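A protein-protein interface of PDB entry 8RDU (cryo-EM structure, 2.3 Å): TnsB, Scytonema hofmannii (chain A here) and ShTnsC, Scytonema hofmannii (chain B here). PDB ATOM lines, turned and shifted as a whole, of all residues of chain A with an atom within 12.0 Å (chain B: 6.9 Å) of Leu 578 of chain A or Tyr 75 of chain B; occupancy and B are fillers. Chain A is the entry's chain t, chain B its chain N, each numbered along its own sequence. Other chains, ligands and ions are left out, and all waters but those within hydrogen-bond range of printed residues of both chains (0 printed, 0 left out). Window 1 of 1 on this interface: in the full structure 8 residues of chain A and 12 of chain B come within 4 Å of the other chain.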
ATOM      1  N   GLU A 571       5.261  -8.873  -2.467  1.00  0.00           N
ATOM      2  CA  GLU A 571       5.825  -7.588  -2.864  1.00  0.00           C
ATOM      3  C   GLU A 571       7.303  -7.722  -3.227  1.00  0.00           C
ATOM      4  O   GLU A 571       7.949  -8.716  -2.895  1.00  0.00           O
ATOM      5  CB  GLU A 571       5.617  -6.544  -1.758  1.00  0.00           C
ATOM      6  CG  GLU A 571       6.502  -6.700  -0.527  1.00  0.00           C
ATOM      7  CD  GLU A 571       5.980  -7.743   0.452  1.00  0.00           C
ATOM      8  OE1 GLU A 571       5.622  -8.856   0.015  1.00  0.00           O
ATOM      9  OE2 GLU A 571       5.917  -7.444   1.662  1.00  0.00           O
ATOM     10  N   VAL A 572       7.824  -6.714  -3.922  1.00  0.00           N
ATOM     11  CA  VAL A 572       9.248  -6.627  -4.228  1.00  0.00           C
ATOM     12  C   VAL A 572      10.007  -6.055  -3.038  1.00  0.00           C
ATOM     13  O   VAL A 572       9.480  -5.261  -2.249  1.00  0.00           O
ATOM     14  CB  VAL A 572       9.480  -5.793  -5.506  1.00  0.00           C
ATOM     15  CG1 VAL A 572       9.301  -4.302  -5.236  1.00  0.00           C
ATOM     16  CG2 VAL A 572      10.850  -6.079  -6.091  1.00  0.00           C
ATOM     17  N   TRP A 573      11.262  -6.483  -2.897  1.00  0.00           N
ATOM     18  CA  TRP A 573      12.189  -5.938  -1.913  1.00  0.00           C
ATOM     19  C   TRP A 573      13.167  -5.037  -2.661  1.00  0.00           C
ATOM     20  O   TRP A 573      13.946  -5.515  -3.488  1.00  0.00           O
ATOM     21  CB  TRP A 573      12.936  -7.067  -1.203  1.00  0.00           C
ATOM     22  CG  TRP A 573      12.057  -8.095  -0.555  1.00  0.00           C
ATOM     23  CD1 TRP A 573      10.810  -7.903  -0.036  1.00  0.00           C
ATOM     24  CD2 TRP A 573      12.345  -9.493  -0.400  1.00  0.00           C
ATOM     25  NE1 TRP A 573      10.314  -9.088   0.454  1.00  0.00           N
ATOM     26  CE2 TRP A 573      11.235 -10.080   0.241  1.00  0.00           C
ATOM     27  CE3 TRP A 573      13.437 -10.303  -0.731  1.00  0.00           C
ATOM     28  CZ2 TRP A 573      11.185 -11.440   0.557  1.00  0.00           C
ATOM     29  CZ3 TRP A 573      13.386 -11.656  -0.416  1.00  0.00           C
ATOM     30  CH2 TRP A 573      12.266 -12.210   0.219  1.00  0.00           C
ATOM     31  N   ASP A 574      13.115  -3.735  -2.396  1.00  0.00           N
ATOM     32  CA  ASP A 574      14.076  -2.831  -3.016  1.00  0.00           C
ATOM     33  C   ASP A 574      15.447  -3.012  -2.375  1.00  0.00           C
ATOM     34  O   ASP A 574      15.570  -3.057  -1.147  1.00  0.00           O
ATOM     35  CB  ASP A 574      13.611  -1.380  -2.887  1.00  0.00           C
ATOM     36  CG  ASP A 574      14.407  -0.426  -3.767  1.00  0.00           C
ATOM     37  OD1 ASP A 574      15.511  -0.789  -4.226  1.00  0.00           O
ATOM     38  OD2 ASP A 574      13.917   0.698  -4.007  1.00  0.00           O
ATOM     39  N   TYR A 575      16.481  -3.129  -3.214  1.00  0.00           N
ATOM     40  CA  TYR A 575      17.842  -3.265  -2.704  1.00  0.00           C
ATOM     41  C   TYR A 575      18.250  -2.066  -1.854  1.00  0.00           C
ATOM     42  O   TYR A 575      18.958  -2.218  -0.851  1.00  0.00           O
ATOM     43  CB  TYR A 575      18.815  -3.429  -3.873  1.00  0.00           C
ATOM     44  CG  TYR A 575      19.787  -4.580  -3.748  1.00  0.00           C
ATOM     45  CD1 TYR A 575      20.646  -4.679  -2.661  1.00  0.00           C
ATOM     46  CD2 TYR A 575      19.863  -5.556  -4.732  1.00  0.00           C
ATOM     47  CE1 TYR A 575      21.535  -5.737  -2.547  1.00  0.00           C
ATOM     48  CE2 TYR A 575      20.750  -6.615  -4.629  1.00  0.00           C
ATOM     49  CZ  TYR A 575      21.583  -6.700  -3.536  1.00  0.00           C
ATOM     50  OH  TYR A 575      22.477  -7.742  -3.438  1.00  0.00           O
ATOM     51  N   GLU A 576      17.811  -0.866  -2.239  1.00  0.00           N
ATOM     52  CA  GLU A 576      18.020   0.320  -1.412  1.00  0.00           C
ATOM     53  C   GLU A 576      17.254   0.261  -0.095  1.00  0.00           C
ATOM     54  O   GLU A 576      17.800   0.600   0.961  1.00  0.00           O
ATOM     55  CB  GLU A 576      17.628   1.572  -2.196  1.00  0.00           C
ATOM     56  CG  GLU A 576      17.781   2.869  -1.417  1.00  0.00           C
ATOM     57  CD  GLU A 576      17.411   4.088  -2.239  1.00  0.00           C
ATOM     58  OE1 GLU A 576      17.806   4.148  -3.422  1.00  0.00           O
ATOM     59  OE2 GLU A 576      16.734   4.990  -1.702  1.00  0.00           O
ATOM     60  N   GLN A 577      15.986  -0.149  -0.138  1.00  0.00           N
ATOM     61  CA  GLN A 577      15.168  -0.167   1.072  1.00  0.00           C
ATOM     62  C   GLN A 577      15.698  -1.154   2.108  1.00  0.00           C
ATOM     63  O   GLN A 577      15.773  -0.829   3.299  1.00  0.00           O
ATOM     64  CB  GLN A 577      13.713  -0.476   0.710  1.00  0.00           C
ATOM     65  CG  GLN A 577      12.757  -0.469   1.892  1.00  0.00           C
ATOM     66  CD  GLN A 577      11.299  -0.493   1.466  1.00  0.00           C
ATOM     67  OE1 GLN A 577      10.987  -0.465   0.273  1.00  0.00           O
ATOM     68  NE2 GLN A 577      10.398  -0.521   2.440  1.00  0.00           N
ATOM     69  N   LEU A 578      16.071  -2.361   1.677  1.00  0.00           N
ATOM     70  CA  LEU A 578      16.643  -3.341   2.599  1.00  0.00           C
ATOM     71  C   LEU A 578      18.001  -2.898   3.134  1.00  0.00           C
ATOM     72  O   LEU A 578      18.343  -3.186   4.288  1.00  0.00           O
ATOM     73  CB  LEU A 578      16.765  -4.699   1.908  1.00  0.00           C
ATOM     74  CG  LEU A 578      15.586  -5.673   1.998  1.00  0.00           C
ATOM     75  CD1 LEU A 578      14.301  -5.057   1.466  1.00  0.00           C
ATOM     76  CD2 LEU A 578      15.906  -6.966   1.266  1.00  0.00           C
ATOM     77  N   ARG A 579      18.799  -2.216   2.309  1.00  0.00           N
ATOM     78  CA  ARG A 579      20.055  -1.651   2.793  1.00  0.00           C
ATOM     79  C   ARG A 579      19.833  -0.549   3.824  1.00  0.00           C
ATOM     80  O   ARG A 579      20.554  -0.479   4.826  1.00  0.00           O
ATOM     81  CB  ARG A 579      20.870  -1.109   1.619  1.00  0.00           C
ATOM     82  CG  ARG A 579      22.275  -0.676   1.994  1.00  0.00           C
ATOM     83  CD  ARG A 579      23.035  -0.112   0.800  1.00  0.00           C
ATOM     84  NE  ARG A 579      23.287  -1.106  -0.237  1.00  0.00           N
ATOM     85  CZ  ARG A 579      23.948  -0.859  -1.361  1.00  0.00           C
ATOM     86  NH1 ARG A 579      24.424   0.346  -1.632  1.00  0.00           N
ATOM     87  NH2 ARG A 579      24.136  -1.844  -2.235  1.00  0.00           N
ATOM     88  N   GLU A 580      18.847   0.324   3.602  1.00  0.00           N
ATOM     89  CA  GLU A 580      18.554   1.363   4.586  1.00  0.00           C
ATOM     90  C   GLU A 580      17.866   0.813   5.830  1.00  0.00           C
ATOM     91  O   GLU A 580      18.168   1.245   6.949  1.00  0.00           O
ATOM     92  CB  GLU A 580      17.707   2.469   3.954  1.00  0.00           C
ATOM     93  CG  GLU A 580      18.439   3.318   2.917  1.00  0.00           C
ATOM     94  CD  GLU A 580      19.604   4.101   3.509  1.00  0.00           C
ATOM     95  OE1 GLU A 580      19.691   4.209   4.751  1.00  0.00           O
ATOM     96  OE2 GLU A 580      20.436   4.610   2.729  1.00  0.00           O
ATOM     97  N   GLU A 581      16.934  -0.128   5.665  1.00  0.00           N
ATOM     98  CA  GLU A 581      16.298  -0.724   6.836  1.00  0.00           C
ATOM     99  C   GLU A 581      17.295  -1.481   7.702  1.00  0.00           C
ATOM    100  O   GLU A 581      17.109  -1.574   8.920  1.00  0.00           O
ATOM    101  CB  GLU A 581      15.149  -1.638   6.410  1.00  0.00           C
ATOM    102  CG  GLU A 581      13.884  -0.891   6.015  1.00  0.00           C
ATOM    103  CD  GLU A 581      12.741  -1.826   5.658  1.00  0.00           C
ATOM    104  OE1 GLU A 581      12.852  -3.037   5.942  1.00  0.00           O
ATOM    105  OE2 GLU A 581      11.732  -1.348   5.097  1.00  0.00           O
ATOM    106  N   TYR A 582      18.346  -2.038   7.094  1.00  0.00           N
ATOM    107  CA  TYR A 582      19.363  -2.753   7.859  1.00  0.00           C
ATOM    108  C   TYR A 582      19.997  -1.880   8.934  1.00  0.00           C
ATOM    109  O   TYR A 582      20.391  -2.389   9.990  1.00  0.00           O
ATOM    110  CB  TYR A 582      20.426  -3.307   6.910  1.00  0.00           C
ATOM    111  CG  TYR A 582      21.007  -4.626   7.361  1.00  0.00           C
ATOM    112  CD1 TYR A 582      20.183  -5.686   7.685  1.00  0.00           C
ATOM    113  CD2 TYR A 582      22.380  -4.824   7.417  1.00  0.00           C
ATOM    114  CE1 TYR A 582      20.700  -6.884   8.108  1.00  0.00           C
ATOM    115  CE2 TYR A 582      22.908  -6.040   7.820  1.00  0.00           C
ATOM    116  CZ  TYR A 582      22.056  -7.066   8.161  1.00  0.00           C
ATOM    117  OH  TYR A 582      22.551  -8.283   8.555  1.00  0.00           O
ATOM    118  N   GLY A 583      20.095  -0.576   8.697  1.00  0.00           N
ATOM    119  CA  GLY A 583      20.666   0.338   9.671  1.00  0.00           C
ATOM    120  C   GLY A 583      19.880   0.386  10.969  1.00  0.00           C
ATOM    121  O   GLY A 583      20.426   0.626  12.045  1.00  0.00           O
ATOM    122  N   ILE B  33      15.324  -6.471  -5.669  1.00  0.00           N
ATOM    123  CA  ILE B  33      15.289  -7.861  -5.220  1.00  0.00           C
ATOM    124  C   ILE B  33      13.858  -8.368  -5.300  1.00  0.00           C
ATOM    125  O   ILE B  33      12.969  -7.857  -4.611  1.00  0.00           O
ATOM    126  CB  ILE B  33      15.819  -8.008  -3.785  1.00  0.00           C
ATOM    127  CG1 ILE B  33      17.194  -7.365  -3.649  1.00  0.00           C
ATOM    128  CG2 ILE B  33      15.832  -9.466  -3.350  1.00  0.00           C
ATOM    129  CD1 ILE B  33      17.810  -7.560  -2.295  1.00  0.00           C
ATOM    130  N   VAL B  68      22.468 -12.551  -4.315  1.00  0.00           N
ATOM    131  CA  VAL B  68      21.283 -11.765  -3.975  1.00  0.00           C
ATOM    132  C   VAL B  68      20.412 -12.476  -2.945  1.00  0.00           C
ATOM    133  O   VAL B  68      19.841 -11.838  -2.053  1.00  0.00           O
ATOM    134  CB  VAL B  68      20.491 -11.426  -5.251  1.00  0.00           C
ATOM    135  CG1 VAL B  68      19.185 -10.759  -4.901  1.00  0.00           C
ATOM    136  CG2 VAL B  68      21.310 -10.520  -6.143  1.00  0.00           C
ATOM    137  N   CYS B  70      21.554 -14.627  -0.649  1.00  0.00           N
ATOM    138  CA  CYS B  70      22.272 -14.552   0.623  1.00  0.00           C
ATOM    139  C   CYS B  70      22.245 -13.156   1.233  1.00  0.00           C
ATOM    140  O   CYS B  70      22.163 -13.017   2.457  1.00  0.00           O
ATOM    141  CB  CYS B  70      23.709 -15.031   0.437  1.00  0.00           C
ATOM    142  SG  CYS B  70      23.870 -16.825   0.302  1.00  0.00           S
ATOM    143  N   ASP B  71      22.332 -12.114   0.410  1.00  0.00           N
ATOM    144  CA  ASP B  71      22.076 -10.761   0.893  1.00  0.00           C
ATOM    145  C   ASP B  71      20.675 -10.625   1.475  1.00  0.00           C
ATOM    146  O   ASP B  71      20.496 -10.050   2.551  1.00  0.00           O
ATOM    147  CB  ASP B  71      22.291  -9.751  -0.230  1.00  0.00           C
ATOM    148  CG  ASP B  71      23.684  -9.169  -0.222  1.00  0.00           C
ATOM    149  OD1 ASP B  71      24.400  -9.364   0.780  1.00  0.00           O
ATOM    150  OD2 ASP B  71      24.071  -8.524  -1.213  1.00  0.00           O
ATOM    151  N   ALA B  72      19.667 -11.139   0.773  1.00  0.00           N
ATOM    152  CA  ALA B  72      18.307 -11.137   1.304  1.00  0.00           C
ATOM    153  C   ALA B  72      18.191 -11.865   2.643  1.00  0.00           C
ATOM    154  O   ALA B  72      17.430 -11.438   3.516  1.00  0.00           O
ATOM    155  CB  ALA B  72      17.356 -11.758   0.282  1.00  0.00           C
ATOM    156  N   TYR B  73      18.916 -12.967   2.828  1.00  0.00           N
ATOM    157  CA  TYR B  73      18.864 -13.670   4.111  1.00  0.00           C
ATOM    158  C   TYR B  73      19.522 -12.867   5.223  1.00  0.00           C
ATOM    159  O   TYR B  73      19.021 -12.819   6.349  1.00  0.00           O
ATOM    160  CB  TYR B  73      19.538 -15.031   4.004  1.00  0.00           C
ATOM    161  CG  TYR B  73      19.347 -15.901   5.219  1.00  0.00           C
ATOM    162  CD1 TYR B  73      18.142 -16.541   5.448  1.00  0.00           C
ATOM    163  CD2 TYR B  73      20.357 -16.063   6.148  1.00  0.00           C
ATOM    164  CE1 TYR B  73      17.965 -17.346   6.541  1.00  0.00           C
ATOM    165  CE2 TYR B  73      20.182 -16.849   7.253  1.00  0.00           C
ATOM    166  CZ  TYR B  73      18.987 -17.487   7.449  1.00  0.00           C
ATOM    167  OH  TYR B  73      18.811 -18.272   8.559  1.00  0.00           O
ATOM    168  N   ARG B  74      20.664 -12.263   4.925  1.00  0.00           N
ATOM    169  CA  ARG B  74      21.358 -11.405   5.875  1.00  0.00           C
ATOM    170  C   ARG B  74      20.523 -10.190   6.275  1.00  0.00           C
ATOM    171  O   ARG B  74      20.508  -9.802   7.448  1.00  0.00           O
ATOM    172  CB  ARG B  74      22.705 -11.018   5.264  1.00  0.00           C
ATOM    173  CG  ARG B  74      23.517 -10.013   5.989  1.00  0.00           C
ATOM    174  CD  ARG B  74      23.327  -8.665   5.366  1.00  0.00           C
ATOM    175  NE  ARG B  74      24.069  -8.565   4.118  1.00  0.00           N
ATOM    176  CZ  ARG B  74      25.046  -7.699   3.902  1.00  0.00           C
ATOM    177  NH1 ARG B  74      25.467  -6.887   4.852  1.00  0.00           N
ATOM    178  NH2 ARG B  74      25.621  -7.654   2.705  1.00  0.00           N
ATOM    179  N   TYR B  75      19.815  -9.583   5.323  1.00  0.00           N
ATOM    180  CA  TYR B  75      18.965  -8.435   5.631  1.00  0.00           C
ATOM    181  C   TYR B  75      17.725  -8.795   6.448  1.00  0.00           C
ATOM    182  O   TYR B  75      17.217  -7.946   7.183  1.00  0.00           O
ATOM    183  CB  TYR B  75      18.576  -7.705   4.349  1.00  0.00           C
ATOM    184  CG  TYR B  75      19.749  -7.033   3.671  1.00  0.00           C
ATOM    185  CD1 TYR B  75      20.668  -6.303   4.409  1.00  0.00           C
ATOM    186  CD2 TYR B  75      19.928  -7.109   2.299  1.00  0.00           C
ATOM    187  CE1 TYR B  75      21.730  -5.679   3.807  1.00  0.00           C
ATOM    188  CE2 TYR B  75      20.993  -6.491   1.686  1.00  0.00           C
ATOM    189  CZ  TYR B  75      21.892  -5.776   2.446  1.00  0.00           C
ATOM    190  OH  TYR B  75      22.960  -5.158   1.841  1.00  0.00           O
ATOM    191  N   ARG B  76      17.222 -10.026   6.352  1.00  0.00           N
ATOM    192  CA  ARG B  76      16.141 -10.426   7.252  1.00  0.00           C
ATOM    193  C   ARG B  76      16.609 -10.664   8.680  1.00  0.00           C
ATOM    194  O   ARG B  76      15.809 -10.553   9.611  1.00  0.00           O
ATOM    195  CB  ARG B  76      15.458 -11.683   6.727  1.00  0.00           C
ATOM    196  CG  ARG B  76      14.655 -11.466   5.468  1.00  0.00           C
ATOM    197  CD  ARG B  76      13.532 -12.482   5.337  1.00  0.00           C
ATOM    198  NE  ARG B  76      13.999 -13.860   5.423  1.00  0.00           N
ATOM    199  CZ  ARG B  76      13.837 -14.651   6.475  1.00  0.00           C
ATOM    200  NH1 ARG B  76      13.265 -14.216   7.586  1.00  0.00           N
ATOM    201  NH2 ARG B  76      14.269 -15.908   6.412  1.00  0.00           N
ATOM    202  N   HIS B  77      17.872 -11.013   8.876  1.00  0.00           N
ATOM    203  CA  HIS B  77      18.430 -11.274  10.202  1.00  0.00           C
ATOM    204  C   HIS B  77      19.380 -10.147  10.597  1.00  0.00           C
ATOM    205  O   HIS B  77      20.603 -10.290  10.593  1.00  0.00           O
ATOM    206  CB  HIS B  77      19.074 -12.635  10.229  1.00  0.00           C
ATOM    207  CG  HIS B  77      18.125 -13.730   9.865  1.00  0.00           C
ATOM    208  ND1 HIS B  77      17.946 -14.166   8.572  1.00  0.00           N
ATOM    209  CD2 HIS B  77      17.280 -14.458  10.630  1.00  0.00           C
ATOM    210  CE1 HIS B  77      17.030 -15.116   8.557  1.00  0.00           C
ATOM    211  NE2 HIS B  77      16.616 -15.319   9.793  1.00  0.00           N
ATOM    212  N   LYS B  78      18.782  -9.007  10.932  1.00  0.00           N
ATOM    213  CA  LYS B  78      19.519  -7.781  11.183  1.00  0.00           C
ATOM    214  C   LYS B  78      20.343  -7.860  12.470  1.00  0.00           C
ATOM    215  O   LYS B  78      19.977  -8.561  13.416  1.00  0.00           O
ATOM    216  CB  LYS B  78      18.558  -6.602  11.276  1.00  0.00           C
ATOM    217  CG  LYS B  78      17.509  -6.581  10.193  1.00  0.00           C
ATOM    218  CD  LYS B  78      16.683  -5.312  10.247  1.00  0.00           C
ATOM    219  CE  LYS B  78      15.376  -5.478   9.490  1.00  0.00           C
ATOM    220  NZ  LYS B  78      15.588  -5.761   8.048  1.00  0.00           N
ATOM    221  N   PRO B  79      21.469  -7.152  12.516  1.00  0.00           N
ATOM    222  CA  PRO B  79      22.044  -6.732  13.796  1.00  0.00           C
ATOM    223  C   PRO B  79      20.992  -6.145  14.722  1.00  0.00           C
ATOM    224  O   PRO B  79      20.237  -5.244  14.350  1.00  0.00           O
ATOM    225  CB  PRO B  79      23.080  -5.680  13.385  1.00  0.00           C
ATOM    226  CG  PRO B  79      23.466  -6.064  12.021  1.00  0.00           C
ATOM    227  CD  PRO B  79      22.212  -6.587  11.383  1.00  0.00           C
ATOM    228  N   VAL B  91      23.697 -13.333  11.841  1.00  0.00           N
ATOM    229  CA  VAL B  91      24.282 -13.720  10.562  1.00  0.00           C
ATOM    230  C   VAL B  91      25.341 -12.700  10.169  1.00  0.00           C
ATOM    231  O   VAL B  91      25.045 -11.509  10.025  1.00  0.00           O
ATOM    232  CB  VAL B  91      23.211 -13.842   9.468  1.00  0.00           C
ATOM    233  CG1 VAL B  91      23.837 -14.258   8.155  1.00  0.00           C
ATOM    234  CG2 VAL B  91      22.148 -14.830   9.882  1.00  0.00           C
ATOM    235  N   TYR B 112      32.918  -6.403  10.005  1.00  0.00           N
ATOM    236  CA  TYR B 112      31.494  -6.537   9.731  1.00  0.00           C
ATOM    237  C   TYR B 112      30.693  -6.298  11.000  1.00  0.00           C
ATOM    238  O   TYR B 112      29.698  -5.567  10.992  1.00  0.00           O
ATOM    239  CB  TYR B 112      31.189  -7.913   9.155  1.00  0.00           C
ATOM    240  CG  TYR B 112      29.750  -8.095   8.762  1.00  0.00           C
ATOM    241  CD1 TYR B 112      28.812  -8.533   9.680  1.00  0.00           C
ATOM    242  CD2 TYR B 112      29.321  -7.802   7.484  1.00  0.00           C
ATOM    243  CE1 TYR B 112      27.512  -8.707   9.326  1.00  0.00           C
ATOM    244  CE2 TYR B 112      28.012  -7.961   7.127  1.00  0.00           C
ATOM    245  CZ  TYR B 112      27.116  -8.420   8.050  1.00  0.00           C
ATOM    246  OH  TYR B 112      25.802  -8.561   7.705  1.00  0.00           O
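N of Ile 33 of chain B sits at hydrogen-bond distance from O of Trp 573 of chain A.
OH of Tyr 575 of chain A lies within hydrogen-bond range of OD2 of Asp 71 of chain B, at 2.8 Å.
The backbone carbonyl oxygen (O) of Arg 74 of chain B lies within hydrogen-bond range of the side-chain hydroxyl (OH) of Tyr 582 of chain A.
The backbone carbonyl oxygen of His 77 of chain B sits at hydrogen-bond distance from the side-chain hydroxyl of Tyr 582 of chain A (3.5 Å).
OH of Tyr 112 of chain B is in hydrogen-bond range of OH of Tyr 582 of chain A (3.4 Å).
The side-chain carboxylate of Asp 71 of chain B is in salt-bridge range of the guanidinium group of Arg 74 of chain B.
A ring nitrogen (ND1) of His 77 of chain B is in hydrogen-bond range of the backbone carbonyl oxygen of Tyr 73 of chain B, 2.8 Å away.
The side-chain hydroxyl of Tyr 112 of chain B lies close to the guanidinium group of Arg 74 of chain B (3.3 Å).
The backbone carbonyl oxygen (O) of Tyr 75 of chain B lies within hydrogen-bond range of the side-chain amino group (NZ) of Lys 78 of chain B.
The side-chain amide nitrogen of Gln 577 of chain A is in hydrogen-bond range of the side-chain carboxylate of Glu 581 of chain A (3.1 Å).
O of Ile 33 of chain B touches CG2 of Val 572 of chain A, at 3.1 Å.
Tyr 575 of chain A touches Ile 33 of chain B.
CD1 of Tyr 75 of chain B touches O of Leu 578 of chain A, at 3.9 Å.
O of Glu 581 of chain A touches CD of Lys 78 of chain B, at 3.99 Å.
Tyr 582 of chain A touches Tyr 75 of chain B.
CA of Lys 78 of chain B touches CE1 of Tyr 582 of chain A, at 3.4 Å.
Tyr 582 of chain A touches Pro 79 of chain B.
Of chain A, only Leu 578 and Tyr 582 come within 4 Å of Tyr 75 of chain B.
Ile 33 of chain B touches just these residues of chain A: Val 572, Trp 573 and Tyr 575.
Asp 71 of chain B touches just one residue of chain A: Tyr 575.
Ala 72 of chain B touches none of the printed residues of chain A.
Of the printed residues of chain A, Arg 74 of chain B touches Tyr 582.
Of the printed residues of chain A, Lys 78 of chain B touches Glu 581 and Tyr 582.
Of the printed residues of chain B, Glu 581 of chain A touches Lys 78.
Of the printed residues of chain B, Tyr 575 of chain A touches Ile 33 (3.4 Å) and Asp 71 (2.8 Å).
Printed residues of chain B within 4 Å of Tyr 582 of chain A: Arg 74 (2.8 Å), Tyr 75 (3.4 Å), His 77 (3.5 Å), Lys 78 (3.4 Å), Pro 79 (3.3 Å) and Tyr 112 (3.4 Å).
Of the printed residues of chain B, Trp 573 of chain A touches Ile 33 (2.8 Å).
The nearest residue of chain A that does not touch Tyr 75 of chain B is Tyr 575 of chain A (4.3 Å).
The nearest printed residue of chain B that does not touch Tyr 582 of chain A is Val 91 of chain B (4.3 Å).
Among the printed residues, 12 pairs touch across the chains.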
